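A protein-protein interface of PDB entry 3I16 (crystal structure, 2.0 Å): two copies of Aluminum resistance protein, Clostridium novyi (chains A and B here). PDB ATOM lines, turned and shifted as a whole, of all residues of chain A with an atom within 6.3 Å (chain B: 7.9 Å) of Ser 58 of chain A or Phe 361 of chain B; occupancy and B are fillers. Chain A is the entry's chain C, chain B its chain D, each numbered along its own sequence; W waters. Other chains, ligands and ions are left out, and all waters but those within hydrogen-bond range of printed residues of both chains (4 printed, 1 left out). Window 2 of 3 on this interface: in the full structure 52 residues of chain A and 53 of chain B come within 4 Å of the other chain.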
ATOM      1  N   GLN A  53     -21.767   6.104  22.059  1.00  0.00           N
ATOM      2  CA  GLN A  53     -22.211   6.037  23.444  1.00  0.00           C
ATOM      3  C   GLN A  53     -23.049   7.234  23.835  1.00  0.00           C
ATOM      4  O   GLN A  53     -24.065   7.080  24.545  1.00  0.00           O
ATOM      5  CB  GLN A  53     -21.010   5.849  24.367  1.00  0.00           C
ATOM      6  CG  GLN A  53     -20.381   4.516  24.146  1.00  0.00           C
ATOM      7  CD  GLN A  53     -19.125   4.297  24.938  1.00  0.00           C
ATOM      8  OE1 GLN A  53     -18.413   5.236  25.248  1.00  0.00           O
ATOM      9  NE2 GLN A  53     -18.825   3.037  25.231  1.00  0.00           N
ATOM     10  N   GLU A  55     -24.970   8.896  21.906  1.00  0.00           N
ATOM     11  CA  GLU A  55     -26.278   8.703  21.284  1.00  0.00           C
ATOM     12  C   GLU A  55     -27.000   7.434  21.773  1.00  0.00           C
ATOM     13  O   GLU A  55     -28.071   7.117  21.285  1.00  0.00           O
ATOM     14  CB  GLU A  55     -26.149   8.720  19.767  1.00  0.00           C
ATOM     15  CG  GLU A  55     -25.798  10.091  19.218  1.00  0.00           C
ATOM     16  CD  GLU A  55     -26.869  11.132  19.492  1.00  0.00           C
ATOM     17  OE1 GLU A  55     -28.073  10.812  19.387  1.00  0.00           O
ATOM     18  OE2 GLU A  55     -26.497  12.281  19.791  1.00  0.00           O
ATOM     19  N   ARG A  56     -26.416   6.740  22.741  1.00  0.00           N
ATOM     20  CA  ARG A  56     -27.003   5.531  23.323  1.00  0.00           C
ATOM     21  C   ARG A  56     -27.484   4.565  22.242  1.00  0.00           C
ATOM     22  O   ARG A  56     -28.618   4.038  22.296  1.00  0.00           O
ATOM     23  CB  ARG A  56     -28.127   5.881  24.314  1.00  0.00           C
ATOM     24  CG  ARG A  56     -27.619   6.521  25.607  1.00  0.00           C
ATOM     25  CD  ARG A  56     -28.753   7.070  26.507  1.00  0.00           C
ATOM     26  NE  ARG A  56     -29.498   6.057  27.257  1.00  0.00           N
ATOM     27  CZ  ARG A  56     -29.266   5.738  28.531  1.00  0.00           C
ATOM     28  NH1 ARG A  56     -28.299   6.339  29.220  1.00  0.00           N
ATOM     29  NH2 ARG A  56     -30.009   4.821  29.129  1.00  0.00           N
ATOM     30  N   ILE A  57     -26.604   4.314  21.268  1.00  0.00           N
ATOM     31  CA  ILE A  57     -26.954   3.425  20.168  1.00  0.00           C
ATOM     32  C   ILE A  57     -27.229   2.008  20.721  1.00  0.00           C
ATOM     33  O   ILE A  57     -26.498   1.502  21.576  1.00  0.00           O
ATOM     34  CB  ILE A  57     -25.904   3.405  19.039  1.00  0.00           C
ATOM     35  CG1 ILE A  57     -25.659   4.815  18.451  1.00  0.00           C
ATOM     36  CG2 ILE A  57     -26.335   2.410  17.938  1.00  0.00           C
ATOM     37  CD1 ILE A  57     -26.897   5.544  17.922  1.00  0.00           C
ATOM     38  N   SER A  58     -28.330   1.421  20.257  1.00  0.00           N
ATOM     39  CA  SER A  58     -28.779   0.107  20.645  1.00  0.00           C
ATOM     40  C   SER A  58     -29.179  -0.672  19.399  1.00  0.00           C
ATOM     41  O   SER A  58     -29.210  -0.120  18.286  1.00  0.00           O
ATOM     42  CB  SER A  58     -30.019   0.211  21.530  1.00  0.00           C
ATOM     43  OG  SER A  58     -31.137   0.601  20.770  1.00  0.00           O
ATOM     44  N   GLU A  59     -29.495  -1.950  19.574  1.00  0.00           N
ATOM     45  CA  GLU A  59     -29.966  -2.766  18.446  1.00  0.00           C
ATOM     46  C   GLU A  59     -31.216  -2.207  17.815  1.00  0.00           C
ATOM     47  O   GLU A  59     -31.461  -2.462  16.648  1.00  0.00           O
ATOM     48  CB  GLU A  59     -30.226  -4.216  18.842  1.00  0.00           C
ATOM     49  CG  GLU A  59     -28.956  -4.977  19.137  1.00  0.00           C
ATOM     50  CD  GLU A  59     -29.091  -6.451  18.819  1.00  0.00           C
ATOM     51  OE1 GLU A  59     -29.181  -6.787  17.605  1.00  0.00           O
ATOM     52  OE2 GLU A  59     -29.046  -7.265  19.776  1.00  0.00           O
ATOM     53  N   ALA A  60     -31.994  -1.443  18.580  1.00  0.00           N
ATOM     54  CA  ALA A  60     -33.173  -0.774  18.067  1.00  0.00           C
ATOM     55  C   ALA A  60     -32.847   0.249  16.971  1.00  0.00           C
ATOM     56  O   ALA A  60     -33.703   0.582  16.188  1.00  0.00           O
ATOM     57  CB  ALA A  60     -33.944  -0.109  19.217  1.00  0.00           C
ATOM     58  N   HIS A  61     -31.622   0.765  16.917  1.00  0.00           N
ATOM     59  CA  HIS A  61     -31.255   1.679  15.854  1.00  0.00           C
ATOM     60  C   HIS A  61     -30.924   0.948  14.554  1.00  0.00           C
ATOM     61  O   HIS A  61     -30.662   1.589  13.549  1.00  0.00           O
ATOM     62  CB  HIS A  61     -30.101   2.577  16.291  1.00  0.00           C
ATOM     63  CG  HIS A  61     -30.469   3.471  17.426  1.00  0.00           C
ATOM     64  ND1 HIS A  61     -30.281   3.116  18.744  1.00  0.00           N
ATOM     65  CD2 HIS A  61     -31.100   4.665  17.444  1.00  0.00           C
ATOM     66  CE1 HIS A  61     -30.758   4.069  19.524  1.00  0.00           C
ATOM     67  NE2 HIS A  61     -31.253   5.026  18.760  1.00  0.00           N
ATOM     68  N   PHE A  62     -30.869  -0.379  14.577  1.00  0.00           N
ATOM     69  CA  PHE A  62     -30.613  -1.117  13.354  1.00  0.00           C
ATOM     70  C   PHE A  62     -31.964  -1.341  12.713  1.00  0.00           C
ATOM     71  O   PHE A  62     -32.480  -2.453  12.724  1.00  0.00           O
ATOM     72  CB  PHE A  62     -29.890  -2.451  13.625  1.00  0.00           C
ATOM     73  CG  PHE A  62     -28.534  -2.291  14.279  1.00  0.00           C
ATOM     74  CD1 PHE A  62     -27.762  -1.131  14.086  1.00  0.00           C
ATOM     75  CD2 PHE A  62     -28.005  -3.329  15.053  1.00  0.00           C
ATOM     76  CE1 PHE A  62     -26.514  -1.013  14.688  1.00  0.00           C
ATOM     77  CE2 PHE A  62     -26.751  -3.208  15.657  1.00  0.00           C
ATOM     78  CZ  PHE A  62     -26.019  -2.054  15.479  1.00  0.00           C
ATOM     79  N   ILE A  73     -35.545   5.987  13.512  1.00  0.00           N
ATOM     80  CA  ILE A  73     -34.551   6.338  14.551  1.00  0.00           C
ATOM     81  C   ILE A  73     -33.139   5.901  14.191  1.00  0.00           C
ATOM     82  O   ILE A  73     -32.172   6.524  14.637  1.00  0.00           O
ATOM     83  CB  ILE A  73     -34.920   5.827  15.973  1.00  0.00           C
ATOM     84  CG1 ILE A  73     -34.822   4.307  16.085  1.00  0.00           C
ATOM     85  CG2 ILE A  73     -36.318   6.332  16.348  1.00  0.00           C
ATOM     86  CD1 ILE A  73     -34.996   3.743  17.570  1.00  0.00           C
ATOM     87  N   GLN B 353     -19.164  -3.716  29.473  1.00  0.00           N
ATOM     88  CA  GLN B 353     -20.428  -3.319  28.844  1.00  0.00           C
ATOM     89  C   GLN B 353     -20.384  -1.827  28.457  1.00  0.00           C
ATOM     90  O   GLN B 353     -20.739  -1.456  27.317  1.00  0.00           O
ATOM     91  CB  GLN B 353     -21.621  -3.578  29.778  1.00  0.00           C
ATOM     92  CG  GLN B 353     -22.979  -3.340  29.154  1.00  0.00           C
ATOM     93  CD  GLN B 353     -23.296  -4.332  28.065  1.00  0.00           C
ATOM     94  OE1 GLN B 353     -23.214  -5.532  28.282  1.00  0.00           O
ATOM     95  NE2 GLN B 353     -23.659  -3.837  26.881  1.00  0.00           N
ATOM     96  N   THR B 354     -19.899  -0.987  29.375  1.00  0.00           N
ATOM     97  CA  THR B 354     -19.831   0.462  29.130  1.00  0.00           C
ATOM     98  C   THR B 354     -18.811   0.838  28.036  1.00  0.00           C
ATOM     99  O   THR B 354     -18.816   1.958  27.539  1.00  0.00           O
ATOM    100  CB  THR B 354     -19.524   1.260  30.410  1.00  0.00           C
ATOM    101  OG1 THR B 354     -18.196   0.977  30.834  1.00  0.00           O
ATOM    102  CG2 THR B 354     -20.527   0.927  31.516  1.00  0.00           C
ATOM    103  N   GLY B 355     -17.926  -0.083  27.688  1.00  0.00           N
ATOM    104  CA  GLY B 355     -16.980   0.127  26.613  1.00  0.00           C
ATOM    105  C   GLY B 355     -17.487  -0.316  25.237  1.00  0.00           C
ATOM    106  O   GLY B 355     -16.745  -0.200  24.254  1.00  0.00           O
ATOM    107  N   SER B 356     -18.734  -0.788  25.140  1.00  0.00           N
ATOM    108  CA  SER B 356     -19.281  -1.287  23.872  1.00  0.00           C
ATOM    109  C   SER B 356     -19.885  -0.147  23.052  1.00  0.00           C
ATOM    110  O   SER B 356     -20.403   0.789  23.613  1.00  0.00           O
ATOM    111  CB  SER B 356     -20.399  -2.294  24.132  1.00  0.00           C
ATOM    112  OG  SER B 356     -19.990  -3.264  25.074  1.00  0.00           O
ATOM    113  N   PRO B 357     -19.827  -0.233  21.721  1.00  0.00           N
ATOM    114  CA  PRO B 357     -20.487   0.774  20.921  1.00  0.00           C
ATOM    115  C   PRO B 357     -22.008   0.635  20.981  1.00  0.00           C
ATOM    116  O   PRO B 357     -22.719   1.643  20.931  1.00  0.00           O
ATOM    117  CB  PRO B 357     -19.985   0.495  19.518  1.00  0.00           C
ATOM    118  CG  PRO B 357     -19.600  -0.931  19.526  1.00  0.00           C
ATOM    119  CD  PRO B 357     -19.100  -1.211  20.897  1.00  0.00           C
ATOM    120  N   ILE B 358     -22.498  -0.603  21.077  1.00  0.00           N
ATOM    121  CA  ILE B 358     -23.947  -0.877  21.141  1.00  0.00           C
ATOM    122  C   ILE B 358     -24.394  -1.246  22.570  1.00  0.00           C
ATOM    123  O   ILE B 358     -23.736  -2.028  23.224  1.00  0.00           O
ATOM    124  CB  ILE B 358     -24.339  -2.044  20.172  1.00  0.00           C
ATOM    125  CG1 ILE B 358     -23.735  -1.843  18.779  1.00  0.00           C
ATOM    126  CG2 ILE B 358     -25.841  -2.192  20.102  1.00  0.00           C
ATOM    127  CD1 ILE B 358     -24.080  -0.511  18.147  1.00  0.00           C
ATOM    128  N   ASP B 359     -25.517  -0.703  23.041  1.00  0.00           N
ATOM    129  CA  ASP B 359     -26.052  -1.036  24.375  1.00  0.00           C
ATOM    130  C   ASP B 359     -25.061  -0.740  25.519  1.00  0.00           C
ATOM    131  O   ASP B 359     -25.057  -1.430  26.546  1.00  0.00           O
ATOM    132  CB  ASP B 359     -26.498  -2.519  24.461  1.00  0.00           C
ATOM    133  CG  ASP B 359     -27.677  -2.835  23.581  1.00  0.00           C
ATOM    134  OD1 ASP B 359     -28.441  -1.919  23.214  1.00  0.00           O
ATOM    135  OD2 ASP B 359     -27.867  -4.022  23.279  1.00  0.00           O
ATOM    136  N   SER B 360     -24.272   0.320  25.357  1.00  0.00           N
ATOM    137  CA  SER B 360     -23.298   0.725  26.360  1.00  0.00           C
ATOM    138  C   SER B 360     -23.942   1.174  27.680  1.00  0.00           C
ATOM    139  O   SER B 360     -23.291   1.181  28.730  1.00  0.00           O
ATOM    140  CB  SER B 360     -22.461   1.875  25.801  1.00  0.00           C
ATOM    141  OG  SER B 360     -23.277   3.024  25.548  1.00  0.00           O
ATOM    142  N   PHE B 361     -25.203   1.578  27.601  1.00  0.00           N
ATOM    143  CA  PHE B 361     -25.991   2.059  28.739  1.00  0.00           C
ATOM    144  C   PHE B 361     -26.807   0.970  29.471  1.00  0.00           C
ATOM    145  O   PHE B 361     -27.514   1.280  30.439  1.00  0.00           O
ATOM    146  CB  PHE B 361     -27.024   3.068  28.219  1.00  0.00           C
ATOM    147  CG  PHE B 361     -27.940   2.490  27.176  1.00  0.00           C
ATOM    148  CD1 PHE B 361     -29.129   1.840  27.536  1.00  0.00           C
ATOM    149  CD2 PHE B 361     -27.612   2.574  25.829  1.00  0.00           C
ATOM    150  CE1 PHE B 361     -29.958   1.289  26.571  1.00  0.00           C
ATOM    151  CE2 PHE B 361     -28.435   2.007  24.862  1.00  0.00           C
ATOM    152  CZ  PHE B 361     -29.613   1.382  25.227  1.00  0.00           C
ATOM    153  N   VAL B 362     -26.741  -0.269  28.992  1.00  0.00           N
ATOM    154  CA  VAL B 362     -27.573  -1.348  29.519  1.00  0.00           C
ATOM    155  C   VAL B 362     -27.153  -1.907  30.876  1.00  0.00           C
ATOM    156  O   VAL B 362     -25.981  -1.894  31.230  1.00  0.00           O
ATOM    157  CB  VAL B 362     -27.678  -2.506  28.492  1.00  0.00           C
ATOM    158  CG1 VAL B 362     -28.173  -3.775  29.144  1.00  0.00           C
ATOM    159  CG2 VAL B 362     -28.605  -2.101  27.365  1.00  0.00           C
ATOM    160  N   SER B 363     -28.154  -2.379  31.631  1.00  0.00           N
ATOM    161  CA  SER B 363     -27.949  -3.001  32.948  1.00  0.00           C
ATOM    162  C   SER B 363     -27.145  -4.284  32.782  1.00  0.00           C
ATOM    163  O   SER B 363     -27.575  -5.209  32.075  1.00  0.00           O
ATOM    164  CB  SER B 363     -29.294  -3.333  33.593  1.00  0.00           C
ATOM    165  OG  SER B 363     -29.097  -4.055  34.796  1.00  0.00           O
ATOM    166  N   CYS B 364     -25.963  -4.333  33.378  1.00  0.00           N
ATOM    167  CA  CYS B 364     -25.116  -5.524  33.258  1.00  0.00           C
ATOM    168  C   CYS B 364     -25.052  -6.107  34.658  1.00  0.00           C
ATOM    169  O   CYS B 364     -24.366  -5.566  35.517  1.00  0.00           O
ATOM    170  CB  CYS B 364     -23.749  -5.137  32.735  1.00  0.00           C
ATOM    171  SG  CYS B 364     -22.627  -6.519  32.589  1.00  0.00           S
ATOM    172  N   ALA B 382     -23.053  -5.819  20.589  1.00  0.00           N
ATOM    173  CA  ALA B 382     -22.491  -6.094  19.280  1.00  0.00           C
ATOM    174  C   ALA B 382     -23.315  -5.624  18.080  1.00  0.00           C
ATOM    175  O   ALA B 382     -24.527  -5.455  18.161  1.00  0.00           O
ATOM    176  CB  ALA B 382     -22.269  -7.637  19.163  1.00  0.00           C
HETATM  177  O   HOH W   1     -30.127  -4.029  21.885  1.00  0.00           O
HETATM  178  O   HOH W   2     -20.041   4.396  28.159  1.00  0.00           O
HETATM  179  O   HOH W   3     -24.695   5.095  26.258  1.00  0.00           O
HETATM  180  O   HOH W   4     -24.390   2.384  22.980  1.00  0.00           O
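Among the printed residues, pairs that only touch across the chains: Ser 58 of chain A with Asp 359 of chain B (3.1 Å), Arg 56 of chain A with Phe 361 of chain B (3.3 Å), Ile 57 of chain A with Ile 358 of chain B (3.5 Å), Gln 53 of chain A with Ser 360 of chain B (3.5 Å), Gln 53 of chain A with Gly 355 of chain B (3.6 Å), Phe 62 of chain A with Ile 358 of chain B (3.6 Å), Glu 59 of chain A with Ile 358 of chain B (3.7 Å), Ser 58 of chain A with Ile 358 of chain B (3.7 Å), Glu 59 of chain A with Asp 359 of chain B (3.8 Å), Ile 57 of chain A with Pro 357 of chain B (3.8 Å), Ile 57 of chain A with Phe 361 of chain B (3.8 Å) and Ser 58 of chain A with Phe 361 of chain B (3.9 Å).
No position is printed for both chains.
Of the printed residues of chain B, Gln 53 of chain A touches Thr 354, Gly 355, Ser 356 and Ser 360.
Printed residues of chain B within 4 Å of Glu 59 of chain A: Ile 358 (3.7 Å) and Asp 359 (3.8 Å).
Of the printed residues of chain A, Gly 355 of chain B touches Gln 53 (3.6 Å).
Printed residues of chain A within 4 Å of Pro 357 of chain B: Ile 57.
Printed residues of chain A within 4 Å of Ser 360 of chain B: Gln 53 (3.5 Å).
Of the printed residues of chain A, Phe 361 of chain B touches Arg 56, Ile 57 and Ser 58.
Hydrophobic or aromatic side chains of chain A within 4 Å of the printed part of chain B: Ile 57 and Phe 62.
Of the 13 printed residues of chain B, 8 touch a printed residue of chain A.
Hydrophobic or aromatic side chains of chain B that line the printed part of chain A: Ile 358 and Phe 361.
Among the printed residues, no Asp or Glu carboxylate lies within 4 Å of a Lys or Arg side-chain nitrogen of the other chain.
The side-chain amide nitrogen (NE2) of Gln 53 of chain A is in hydrogen-bond range of the backbone carbonyl oxygen (O) of Thr 354 of chain B (2.5 Å).
NE2 of Gln 53 of chain A is in hydrogen-bond range of O of Ser 356 of chain B, 3.2 Å away.
The backbone carbonyl oxygen (O) of Ile 57 of chain A is in hydrogen-bond range of the backbone NH (N) of Asp 359 of chain B (2.8 Å).
Water W3 lies within hydrogen-bond range of OG of Ser 360 of chain B (2.6 Å) and O of Gln 53 of chain A (2.7 Å).
Water W1 bridges OD2 of Asp 359 of chain B (2.7 Å) and N of Glu 59 of chain A (3.2 Å).
Water W4 lies within hydrogen-bond range of O of Ile 57 of chain A (2.7 Å), O of Pro 357 of chain B (2.7 Å), OG of Ser 360 of chain B (2.9 Å) and N of Asp 359 of chain B (3.3 Å).
Water W2 lies within hydrogen-bond range of O of Thr 354 of chain B (2.8 Å) and OE1 of Gln 53 of chain A (3.4 Å).
The side-chain hydroxyl of Ser 58 of chain A lies close to the backbone NH of Ala 60 of chain A (3.1 Å).
N of Ser 58 of chain A lies within hydrogen-bond range of ND1 of His 61 of chain A (3.0 Å).
The backbone carbonyl oxygen (O) of Gln 353 of chain B lies within hydrogen-bond range of the side-chain hydroxyl (OG) of Ser 356 of chain B (3.0 Å).
NE2 of Gln 353 of chain B is in hydrogen-bond range of O of Asp 359 of chain B, at 2.8 Å.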
